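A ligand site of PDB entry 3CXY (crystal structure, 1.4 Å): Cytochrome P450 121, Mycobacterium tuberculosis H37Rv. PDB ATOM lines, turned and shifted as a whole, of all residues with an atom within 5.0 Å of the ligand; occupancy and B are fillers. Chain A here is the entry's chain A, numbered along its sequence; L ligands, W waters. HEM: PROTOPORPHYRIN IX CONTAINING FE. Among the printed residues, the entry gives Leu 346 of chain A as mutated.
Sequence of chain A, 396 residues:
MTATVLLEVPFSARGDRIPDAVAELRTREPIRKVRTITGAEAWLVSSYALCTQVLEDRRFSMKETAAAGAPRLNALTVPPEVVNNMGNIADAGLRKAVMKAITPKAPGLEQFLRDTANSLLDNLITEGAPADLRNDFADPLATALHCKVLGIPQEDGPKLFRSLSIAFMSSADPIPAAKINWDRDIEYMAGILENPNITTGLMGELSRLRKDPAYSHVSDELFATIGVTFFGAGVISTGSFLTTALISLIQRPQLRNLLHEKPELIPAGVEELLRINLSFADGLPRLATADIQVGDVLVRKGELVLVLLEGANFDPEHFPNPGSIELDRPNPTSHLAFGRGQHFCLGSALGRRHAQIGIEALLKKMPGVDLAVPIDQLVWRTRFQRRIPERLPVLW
Water W5 bridges O2D of the ligand (3.2 Å) and SD of Met 62 (3.6 Å).
Water W2 lies within hydrogen-bond range of the backbone NH (N) of Met 86 (3.0 Å), an oxygen (O2D) of the ligand (3.3 Å) and the side-chain sulfur (SD) of Met 62 (3.6 Å).
O1A of the ligand lies within salt-bridge range of NH2 of Arg 286 (2.8 Å).
An oxygen (O1D) of the ligand sits at hydrogen-bond distance from a ring nitrogen (ND1) of His 343, at 2.7 Å.
An iron atom (FE) of the ligand is bound by the side-chain sulfur of Cys 345 (2.3 Å).
O2D of the ligand lies close to SD of Met 62 (3.4 Å).
Met 86 touches the ligand.
His 146 touches the ligand (NE2 to CMC, 3.4 Å).
Phe 230 touches the ligand (CZ to CMD, 3.5 Å).
Gly 234 touches the ligand.
Ser 237 touches the ligand.
CG2 of Thr 238 touches CMC of the ligand, at 3.7 Å.
CD2 of Phe 241 touches CBB of the ligand, 3.7 Å away.
Leu 274 touches the ligand.
Phe 280 touches the ligand (CE1 to CHB, 3.6 Å).
Leu 284 touches the ligand (CD1 to CGA, 3.7 Å).
Leu 309 touches the ligand.
Ala 337 touches the ligand.
CE1 of Phe 338 touches C2B of the ligand, at 3.6 Å.
Gly 339 touches the ligand (N to CMA, 3.5 Å).
Gln 342 touches the ligand.
Gly 347 touches the ligand (CA to C3C, 3.7 Å).
Of the 29 residues printed, 20 come within 4 Å of the ligand.
ND1 of His 343 is in hydrogen-bond range of SD of Met 62, 3.6 Å away.
O of Ala 233 lies within hydrogen-bond range of OG of Ser 237 (2.6 Å).
O of Leu 274 sits at hydrogen-bond distance from ND2 of Asn 277 (2.8 Å).
The side-chain hydroxyl (OG1) of Thr 238 sits at hydrogen-bond distance from the backbone carbonyl oxygen (O) of Gly 234, at 2.7 Å.
The backbone NH (N) of Cys 345 is in hydrogen-bond range of the backbone carbonyl oxygen (O) of Phe 338, at 2.8 Å.
SG of Cys 345 sits close to N of Gly 347, 3.3 Å away.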
ATOM      1  N   LEU A  55      17.084  21.946  18.046  1.00  0.00           N
ATOM      2  CA  LEU A  55      18.120  21.267  17.278  1.00  0.00           C
ATOM      3  C   LEU A  55      18.664  20.010  17.973  1.00  0.00           C
ATOM      4  O   LEU A  55      19.156  19.109  17.304  1.00  0.00           O
ATOM      5  CB  LEU A  55      19.265  22.217  16.928  1.00  0.00           C
ATOM      6  CG  LEU A  55      18.933  23.354  15.959  1.00  0.00           C
ATOM      7  CD1 LEU A  55      20.130  24.251  15.782  1.00  0.00           C
ATOM      8  CD2 LEU A  55      18.461  22.791  14.629  1.00  0.00           C
ATOM      9  N   MET A  62      14.656  16.420  10.591  1.00  0.00           N
ATOM     10  CA  MET A  62      15.005  16.923   9.253  1.00  0.00           C
ATOM     11  C   MET A  62      14.395  16.051   8.154  1.00  0.00           C
ATOM     12  O   MET A  62      13.769  16.529   7.200  1.00  0.00           O
ATOM     13  CB  MET A  62      16.536  16.988   9.054  1.00  0.00           C
ATOM     14  CG  MET A  62      16.958  17.304   7.588  1.00  0.00           C
ATOM     15  SD  MET A  62      18.730  17.307   7.396  1.00  0.00           S
ATOM     16  CE  MET A  62      19.113  18.871   8.151  1.00  0.00           C
ATOM     17  N   MET A  86      22.588  12.607   4.864  1.00  0.00           N
ATOM     18  CA  MET A  86      23.545  12.175   5.892  1.00  0.00           C
ATOM     19  C   MET A  86      23.161  10.840   6.574  1.00  0.00           C
ATOM     20  O   MET A  86      24.032  10.023   6.907  1.00  0.00           O
ATOM     21  CB  MET A  86      23.785  13.294   6.906  1.00  0.00           C
ATOM     22  CG  MET A  86      24.740  14.383   6.376  1.00  0.00           C
ATOM     23  SD  MET A  86      26.388  13.806   5.921  1.00  0.00           S
ATOM     24  CE  MET A  86      26.768  12.685   7.277  1.00  0.00           C
ATOM     25  N   ILE A 102      36.997  15.681   3.975  1.00  0.00           N
ATOM     26  CA  ILE A 102      36.656  17.106   3.978  1.00  0.00           C
ATOM     27  C   ILE A 102      37.294  17.936   5.108  1.00  0.00           C
ATOM     28  O   ILE A 102      36.878  19.061   5.364  1.00  0.00           O
ATOM     29  CB  ILE A 102      35.124  17.329   3.952  1.00  0.00           C
ATOM     30  CG1 ILE A 102      34.469  16.791   5.223  1.00  0.00           C
ATOM     31  CG2 ILE A 102      34.522  16.681   2.689  1.00  0.00           C
ATOM     32  CD1 ILE A 102      32.996  17.129   5.338  1.00  0.00           C
ATOM     33  N   HIS A 146      36.537  23.381  -3.471  1.00  0.00           N
ATOM     34  CA  HIS A 146      35.716  22.173  -3.499  1.00  0.00           C
ATOM     35  C   HIS A 146      36.070  21.234  -4.628  1.00  0.00           C
ATOM     36  O   HIS A 146      35.929  20.018  -4.479  1.00  0.00           O
ATOM     37  CB  HIS A 146      34.218  22.540  -3.411  1.00  0.00           C
ATOM     38  CG  HIS A 146      33.838  22.977  -2.044  1.00  0.00           C
ATOM     39  ND1 HIS A 146      34.103  24.258  -1.558  1.00  0.00           N
ATOM     40  CD2 HIS A 146      33.342  22.277  -0.995  1.00  0.00           C
ATOM     41  CE1 HIS A 146      33.752  24.321  -0.297  1.00  0.00           C
ATOM     42  NE2 HIS A 146      33.287  23.139   0.080  1.00  0.00           N
ATOM     43  N   PHE A 230      27.744  17.525  -1.664  1.00  0.00           N
ATOM     44  CA  PHE A 230      28.847  18.137  -0.932  1.00  0.00           C
ATOM     45  C   PHE A 230      29.457  19.326  -1.691  1.00  0.00           C
ATOM     46  O   PHE A 230      29.764  20.371  -1.106  1.00  0.00           O
ATOM     47  CB  PHE A 230      29.877  17.061  -0.492  1.00  0.00           C
ATOM     48  CG  PHE A 230      29.520  16.409   0.819  1.00  0.00           C
ATOM     49  CD1 PHE A 230      28.410  15.560   0.921  1.00  0.00           C
ATOM     50  CD2 PHE A 230      30.250  16.688   1.970  1.00  0.00           C
ATOM     51  CE1 PHE A 230      28.076  14.979   2.139  1.00  0.00           C
ATOM     52  CE2 PHE A 230      29.915  16.129   3.183  1.00  0.00           C
ATOM     53  CZ  PHE A 230      28.829  15.270   3.274  1.00  0.00           C
ATOM     54  N   ALA A 233      26.580  22.244  -1.277  1.00  0.00           N
ATOM     55  CA  ALA A 233      26.424  22.775   0.080  1.00  0.00           C
ATOM     56  C   ALA A 233      27.712  23.489   0.491  1.00  0.00           C
ATOM     57  O   ALA A 233      27.650  24.590   1.041  1.00  0.00           O
ATOM     58  CB  ALA A 233      26.075  21.680   1.051  1.00  0.00           C
ATOM     59  N   GLY A 234      28.859  22.891   0.174  1.00  0.00           N
ATOM     60  CA  GLY A 234      30.110  23.500   0.560  1.00  0.00           C
ATOM     61  C   GLY A 234      30.385  24.789  -0.175  1.00  0.00           C
ATOM     62  O   GLY A 234      30.762  25.775   0.438  1.00  0.00           O
ATOM     63  N   SER A 237      27.873  27.553   0.783  1.00  0.00           N
ATOM     64  CA  SER A 237      27.931  27.949   2.175  1.00  0.00           C
ATOM     65  C   SER A 237      29.204  28.757   2.440  1.00  0.00           C
ATOM     66  O   SER A 237      29.160  29.763   3.127  1.00  0.00           O
ATOM     67  CB  SER A 237      27.883  26.733   3.102  1.00  0.00           C
ATOM     68  OG  SER A 237      26.672  26.005   2.965  1.00  0.00           O
ATOM     69  N   THR A 238      30.329  28.293   1.901  1.00  0.00           N
ATOM     70  CA  THR A 238      31.598  29.002   2.098  1.00  0.00           C
ATOM     71  C   THR A 238      31.676  30.300   1.295  1.00  0.00           C
ATOM     72  O   THR A 238      32.149  31.339   1.793  1.00  0.00           O
ATOM     73  CB  THR A 238      32.819  28.105   1.764  1.00  0.00           C
ATOM     74  OG1 THR A 238      32.735  27.637   0.422  1.00  0.00           O
ATOM     75  CG2 THR A 238      32.935  26.957   2.740  1.00  0.00           C
ATOM     76  N   PHE A 241      29.224  32.765   3.018  1.00  0.00           N
ATOM     77  CA  PHE A 241      29.690  33.198   4.308  1.00  0.00           C
ATOM     78  C   PHE A 241      30.857  34.162   4.149  1.00  0.00           C
ATOM     79  O   PHE A 241      30.877  35.245   4.757  1.00  0.00           O
ATOM     80  CB  PHE A 241      30.126  32.050   5.221  1.00  0.00           C
ATOM     81  CG  PHE A 241      30.858  32.557   6.423  1.00  0.00           C
ATOM     82  CD1 PHE A 241      30.214  33.370   7.324  1.00  0.00           C
ATOM     83  CD2 PHE A 241      32.205  32.297   6.592  1.00  0.00           C
ATOM     84  CE1 PHE A 241      30.897  33.920   8.388  1.00  0.00           C
ATOM     85  CE2 PHE A 241      32.888  32.847   7.657  1.00  0.00           C
ATOM     86  CZ  PHE A 241      32.236  33.652   8.546  1.00  0.00           C
ATOM     87  N   LEU A 274      31.448  34.421  12.034  1.00  0.00           N
ATOM     88  CA  LEU A 274      30.505  33.313  11.971  1.00  0.00           C
ATOM     89  C   LEU A 274      29.316  33.575  12.866  1.00  0.00           C
ATOM     90  O   LEU A 274      28.163  33.421  12.455  1.00  0.00           O
ATOM     91  CB  LEU A 274      31.177  32.008  12.375  1.00  0.00           C
ATOM     92  CG  LEU A 274      32.012  31.378  11.279  1.00  0.00           C
ATOM     93  CD1 LEU A 274      32.962  30.317  11.826  1.00  0.00           C
ATOM     94  CD2 LEU A 274      31.141  30.737  10.173  1.00  0.00           C
ATOM     95  N   ASN A 277      26.920  36.130  11.478  1.00  0.00           N
ATOM     96  CA  ASN A 277      26.630  35.984  10.032  1.00  0.00           C
ATOM     97  C   ASN A 277      25.161  35.768   9.752  1.00  0.00           C
ATOM     98  O   ASN A 277      24.481  35.033  10.443  1.00  0.00           O
ATOM     99  CB  ASN A 277      27.501  34.882   9.389  1.00  0.00           C
ATOM    100  CG  ASN A 277      26.788  33.588   9.159  1.00  0.00           C
ATOM    101  OD1 ASN A 277      26.084  33.448   8.163  1.00  0.00           O
ATOM    102  ND2 ASN A 277      26.990  32.594  10.048  1.00  0.00           N
ATOM    103  N   PHE A 280      22.401  32.451   6.235  1.00  0.00           N
ATOM    104  CA  PHE A 280      21.197  31.611   6.069  1.00  0.00           C
ATOM    105  C   PHE A 280      19.957  32.492   6.006  1.00  0.00           C
ATOM    106  O   PHE A 280      19.645  33.209   6.946  1.00  0.00           O
ATOM    107  CB  PHE A 280      21.060  30.548   7.159  1.00  0.00           C
ATOM    108  CG  PHE A 280      21.832  29.291   6.860  1.00  0.00           C
ATOM    109  CD1 PHE A 280      23.225  29.331   6.765  1.00  0.00           C
ATOM    110  CD2 PHE A 280      21.202  28.083   6.644  1.00  0.00           C
ATOM    111  CE1 PHE A 280      23.955  28.188   6.469  1.00  0.00           C
ATOM    112  CE2 PHE A 280      21.941  26.926   6.343  1.00  0.00           C
ATOM    113  CZ  PHE A 280      23.301  26.990   6.264  1.00  0.00           C
ATOM    114  N   LEU A 284      16.256  27.060   9.936  1.00  0.00           N
ATOM    115  CA  LEU A 284      16.438  25.657   9.616  1.00  0.00           C
ATOM    116  C   LEU A 284      15.130  24.905   9.871  1.00  0.00           C
ATOM    117  O   LEU A 284      14.582  24.971  10.957  1.00  0.00           O
ATOM    118  CB  LEU A 284      17.545  25.062  10.518  1.00  0.00           C
ATOM    119  CG  LEU A 284      18.917  25.714  10.449  1.00  0.00           C
ATOM    120  CD1 LEU A 284      19.901  25.010  11.404  1.00  0.00           C
ATOM    121  CD2 LEU A 284      19.469  25.767   9.045  1.00  0.00           C
ATOM    122  N   ARG A 286      12.445  21.845  10.534  1.00  0.00           N
ATOM    123  CA  ARG A 286      12.261  20.535  11.156  1.00  0.00           C
ATOM    124  C   ARG A 286      10.774  20.250  11.211  1.00  0.00           C
ATOM    125  O   ARG A 286       9.975  21.173  11.331  1.00  0.00           O
ATOM    126  CB  ARG A 286      12.802  20.540  12.598  1.00  0.00           C
ATOM    127  CG  ARG A 286      14.299  20.800  12.726  1.00  0.00           C
ATOM    128  CD  ARG A 286      15.096  19.657  12.161  1.00  0.00           C
ATOM    129  NE  ARG A 286      16.518  19.722  12.499  1.00  0.00           N
ATOM    130  CZ  ARG A 286      17.456  20.288  11.746  1.00  0.00           C
ATOM    131  NH1 ARG A 286      17.134  20.893  10.609  1.00  0.00           N
ATOM    132  NH2 ARG A 286      18.728  20.255  12.156  1.00  0.00           N
ATOM    133  N   LEU A 309      18.692  31.017  13.051  1.00  0.00           N
ATOM    134  CA  LEU A 309      20.072  31.035  13.568  1.00  0.00           C
ATOM    135  C   LEU A 309      20.464  32.380  14.155  1.00  0.00           C
ATOM    136  O   LEU A 309      21.132  32.430  15.210  1.00  0.00           O
ATOM    137  CB  LEU A 309      21.061  30.594  12.513  1.00  0.00           C
ATOM    138  CG  LEU A 309      20.853  29.170  11.992  1.00  0.00           C
ATOM    139  CD1 LEU A 309      21.909  28.822  10.965  1.00  0.00           C
ATOM    140  CD2 LEU A 309      20.756  28.104  13.120  1.00  0.00           C
ATOM    141  N   LEU A 336      25.459  29.069  16.858  1.00  0.00           N
ATOM    142  CA  LEU A 336      24.787  28.076  16.023  1.00  0.00           C
ATOM    143  C   LEU A 336      24.999  28.267  14.512  1.00  0.00           C
ATOM    144  O   LEU A 336      24.200  27.789  13.705  1.00  0.00           O
ATOM    145  CB  LEU A 336      23.287  28.038  16.327  1.00  0.00           C
ATOM    146  CG  LEU A 336      22.875  27.891  17.805  1.00  0.00           C
ATOM    147  CD1 LEU A 336      21.362  27.664  17.937  1.00  0.00           C
ATOM    148  CD2 LEU A 336      23.662  26.819  18.521  1.00  0.00           C
ATOM    149  N   ALA A 337      26.070  28.964  14.122  1.00  0.00           N
ATOM    150  CA  ALA A 337      26.335  29.171  12.684  1.00  0.00           C
ATOM    151  C   ALA A 337      26.473  27.865  11.910  1.00  0.00           C
ATOM    152  O   ALA A 337      26.215  27.860  10.709  1.00  0.00           O
ATOM    153  CB  ALA A 337      27.576  30.026  12.456  1.00  0.00           C
ATOM    154  N   PHE A 338      26.912  26.797  12.579  1.00  0.00           N
ATOM    155  CA  PHE A 338      27.102  25.480  11.959  1.00  0.00           C
ATOM    156  C   PHE A 338      26.014  24.492  12.405  1.00  0.00           C
ATOM    157  O   PHE A 338      26.157  23.262  12.207  1.00  0.00           O
ATOM    158  CB  PHE A 338      28.488  24.926  12.315  1.00  0.00           C
ATOM    159  CG  PHE A 338      29.629  25.654  11.650  1.00  0.00           C
ATOM    160  CD1 PHE A 338      29.711  25.720  10.270  1.00  0.00           C
ATOM    161  CD2 PHE A 338      30.644  26.237  12.399  1.00  0.00           C
ATOM    162  CE1 PHE A 338      30.762  26.358   9.655  1.00  0.00           C
ATOM    163  CE2 PHE A 338      31.710  26.879  11.778  1.00  0.00           C
ATOM    164  CZ  PHE A 338      31.773  26.932  10.403  1.00  0.00           C
ATOM    165  N   GLY A 339      24.937  25.024  12.970  1.00  0.00           N
ATOM    166  CA  GLY A 339      23.913  24.169  13.532  1.00  0.00           C
ATOM    167  C   GLY A 339      24.326  23.605  14.881  1.00  0.00           C
ATOM    168  O   GLY A 339      25.191  24.146  15.569  1.00  0.00           O
ATOM    169  N   GLN A 342      22.369  16.456  15.795  1.00  0.00           N
ATOM    170  CA  GLN A 342      22.535  15.384  14.818  1.00  0.00           C
ATOM    171  C   GLN A 342      23.072  15.911  13.494  1.00  0.00           C
ATOM    172  O   GLN A 342      23.894  15.269  12.843  1.00  0.00           O
ATOM    173  CB  GLN A 342      21.188  14.693  14.577  1.00  0.00           C
ATOM    174  CG  GLN A 342      21.196  13.625  13.518  1.00  0.00           C
ATOM    175  CD  GLN A 342      21.732  12.293  13.995  1.00  0.00           C
ATOM    176  OE1 GLN A 342      21.813  11.331  13.214  1.00  0.00           O
ATOM    177  NE2 GLN A 342      22.092  12.218  15.264  1.00  0.00           N
ATOM    178  N   HIS A 343      22.610  17.090  13.088  1.00  0.00           N
ATOM    179  CA  HIS A 343      22.939  17.612  11.782  1.00  0.00           C
ATOM    180  C   HIS A 343      23.970  18.746  11.775  1.00  0.00           C
ATOM    181  O   HIS A 343      24.076  19.473  10.788  1.00  0.00           O
ATOM    182  CB  HIS A 343      21.649  18.043  11.073  1.00  0.00           C
ATOM    183  CG  HIS A 343      20.686  16.914  10.887  1.00  0.00           C
ATOM    184  ND1 HIS A 343      20.870  15.934   9.942  1.00  0.00           N
ATOM    185  CD2 HIS A 343      19.560  16.589  11.560  1.00  0.00           C
ATOM    186  CE1 HIS A 343      19.883  15.057  10.032  1.00  0.00           C
ATOM    187  NE2 HIS A 343      19.072  15.435  11.005  1.00  0.00           N
ATOM    188  N   PHE A 344      24.760  18.846  12.856  1.00  0.00           N
ATOM    189  CA  PHE A 344      25.890  19.772  12.898  1.00  0.00           C
ATOM    190  C   PHE A 344      26.733  19.676  11.627  1.00  0.00           C
ATOM    191  O   PHE A 344      27.041  18.578  11.126  1.00  0.00           O
ATOM    192  CB  PHE A 344      26.769  19.458  14.112  1.00  0.00           C
ATOM    193  CG  PHE A 344      27.890  20.450  14.301  1.00  0.00           C
ATOM    194  CD1 PHE A 344      27.657  21.627  14.978  1.00  0.00           C
ATOM    195  CD2 PHE A 344      29.146  20.206  13.777  1.00  0.00           C
ATOM    196  CE1 PHE A 344      28.673  22.562  15.149  1.00  0.00           C
ATOM    197  CE2 PHE A 344      30.176  21.156  13.928  1.00  0.00           C
ATOM    198  CZ  PHE A 344      29.927  22.317  14.603  1.00  0.00           C
ATOM    199  N   CYS A 345      27.106  20.842  11.086  1.00  0.00           N
ATOM    200  CA  CYS A 345      27.844  20.928   9.834  1.00  0.00           C
ATOM    201  C   CYS A 345      29.063  20.016   9.765  1.00  0.00           C
ATOM    202  O   CYS A 345      29.975  20.170  10.575  1.00  0.00           O
ATOM    203  CB  CYS A 345      28.292  22.374   9.602  1.00  0.00           C
ATOM    204  SG  CYS A 345      29.104  22.562   8.018  1.00  0.00           S
ATOM    205  N   LEU A 346      29.080  19.112   8.816  1.00  0.00           N
ATOM    206  CA  LEU A 346      30.228  18.220   8.617  1.00  0.00           C
ATOM    207  C   LEU A 346      31.445  19.015   8.142  1.00  0.00           C
ATOM    208  O   LEU A 346      32.589  18.601   8.354  1.00  0.00           O
ATOM    209  CB  LEU A 346      29.921  17.127   7.594  1.00  0.00           C
ATOM    210  CG  LEU A 346      29.147  15.849   7.960  1.00  0.00           C
ATOM    211  CD1 LEU A 346      29.754  14.701   7.148  1.00  0.00           C
ATOM    212  CD2 LEU A 346      29.183  15.506   9.445  1.00  0.00           C
ATOM    213  N   GLY A 347      31.204  20.122   7.454  1.00  0.00           N
ATOM    214  CA  GLY A 347      32.286  20.910   6.863  1.00  0.00           C
ATOM    215  C   GLY A 347      32.777  22.081   7.700  1.00  0.00           C
ATOM    216  O   GLY A 347      33.443  22.961   7.180  1.00  0.00           O
ATOM    217  N   LEU A 350      36.549  22.970   7.545  1.00  0.00           N
ATOM    218  CA  LEU A 350      36.867  23.453   6.210  1.00  0.00           C
ATOM    219  C   LEU A 350      36.327  24.865   5.954  1.00  0.00           C
ATOM    220  O   LEU A 350      36.996  25.695   5.337  1.00  0.00           O
ATOM    221  CB  LEU A 350      36.307  22.491   5.182  1.00  0.00           C
ATOM    222  CG  LEU A 350      36.733  22.644   3.730  1.00  0.00           C
ATOM    223  CD1 LEU A 350      38.270  22.559   3.575  1.00  0.00           C
ATOM    224  CD2 LEU A 350      36.035  21.609   2.894  1.00  0.00           C
ATOM    225  N   GLY A 351      35.107  25.124   6.412  1.00  0.00           N
ATOM    226  CA  GLY A 351      34.501  26.431   6.317  1.00  0.00           C
ATOM    227  C   GLY A 351      35.307  27.484   7.060  1.00  0.00           C
ATOM    228  O   GLY A 351      35.525  28.594   6.559  1.00  0.00           O
HETATM  229  CHA HEM L   1      25.039  21.235   7.760  1.00  0.00           C
HETATM  230  CHB HEM L   1      26.349  25.923   7.839  1.00  0.00           C
HETATM  231  CHC HEM L   1      30.244  24.812   5.140  1.00  0.00           C
HETATM  232  CHD HEM L   1      28.456  20.419   4.344  1.00  0.00           C
HETATM  233  C1A HEM L   1      25.054  22.581   8.059  1.00  0.00           C
HETATM  234  C2A HEM L   1      24.147  23.291   8.925  1.00  0.00           C
HETATM  235  C3A HEM L   1      24.512  24.590   8.932  1.00  0.00           C
HETATM  236  C4A HEM L   1      25.681  24.747   8.082  1.00  0.00           C
HETATM  237  CMA HEM L   1      23.819  25.726   9.692  1.00  0.00           C
HETATM  238  CAA HEM L   1      22.972  22.658   9.688  1.00  0.00           C
HETATM  239  CBA HEM L   1      21.755  22.425   8.798  1.00  0.00           C
HETATM  240  CGA HEM L   1      20.590  21.909   9.606  1.00  0.00           C
HETATM  241  O1A HEM L   1      20.805  21.421  10.764  1.00  0.00           O
HETATM  242  O2A HEM L   1      19.418  21.940   9.104  1.00  0.00           O
HETATM  243  C1B HEM L   1      27.549  26.012   7.146  1.00  0.00           C
HETATM  244  C2B HEM L   1      28.374  27.200   7.049  1.00  0.00           C
HETATM  245  C3B HEM L   1      29.441  26.887   6.303  1.00  0.00           C
HETATM  246  C4B HEM L   1      29.327  25.498   5.908  1.00  0.00           C
HETATM  247  CMB HEM L   1      28.030  28.559   7.710  1.00  0.00           C
HETATM  248  CAB HEM L   1      30.636  27.772   5.920  1.00  0.00           C
HETATM  249  CBB HEM L   1      31.074  28.725   6.728  1.00  0.00           C
HETATM  250  C1C HEM L   1      30.103  23.529   4.713  1.00  0.00           C
HETATM  251  C2C HEM L   1      31.046  22.796   3.877  1.00  0.00           C
HETATM  252  C3C HEM L   1      30.515  21.582   3.668  1.00  0.00           C
HETATM  253  C4C HEM L   1      29.257  21.515   4.355  1.00  0.00           C
HETATM  254  CMC HEM L   1      32.395  23.334   3.365  1.00  0.00           C
HETATM  255  CAC HEM L   1      31.092  20.393   2.864  1.00  0.00           C
HETATM  256  CBC HEM L   1      32.134  20.526   2.046  1.00  0.00           C
HETATM  257  C1D HEM L   1      27.357  20.264   5.144  1.00  0.00           C
HETATM  258  C2D HEM L   1      26.497  19.112   5.068  1.00  0.00           C
HETATM  259  C3D HEM L   1      25.441  19.355   6.139  1.00  0.00           C
HETATM  260  C4D HEM L   1      25.755  20.634   6.743  1.00  0.00           C
HETATM  261  CMD HEM L   1      26.650  17.907   4.115  1.00  0.00           C
HETATM  262  CAD HEM L   1      24.256  18.441   6.477  1.00  0.00           C
HETATM  263  CBD HEM L   1      24.431  17.777   7.832  1.00  0.00           C
HETATM  264  CGD HEM L   1      23.225  16.912   8.130  1.00  0.00           C
HETATM  265  O1D HEM L   1      23.387  15.996   8.965  1.00  0.00           O
HETATM  266  O2D HEM L   1      22.126  17.115   7.554  1.00  0.00           O
HETATM  267  NA  HEM L   1      25.974  23.492   7.565  1.00  0.00           N
HETATM  268  NB  HEM L   1      28.148  25.013   6.420  1.00  0.00           N
HETATM  269  NC  HEM L   1      29.040  22.715   4.989  1.00  0.00           N
HETATM  270  ND  HEM L   1      26.893  21.141   6.135  1.00  0.00           N
HETATM  271 FE   HEM L   1      27.567  23.064   6.369  1.00  0.00          FE
HETATM  272  O   HOH W   1      24.943  15.159   3.286  1.00  0.00           O
HETATM  273  O   HOH W   2      20.658  14.750   5.731  1.00  0.00           O
HETATM  274  O   HOH W   3      22.149  21.350  13.122  1.00  0.00           O
HETATM  275  O   HOH W   4      26.123  23.696   4.619  1.00  0.00           O
HETATM  276  O   HOH W   5      21.024  18.741   5.070  1.00  0.00           O
HETATM  277  O   HOH W   6      18.605  22.521   6.702  1.00  0.00           O
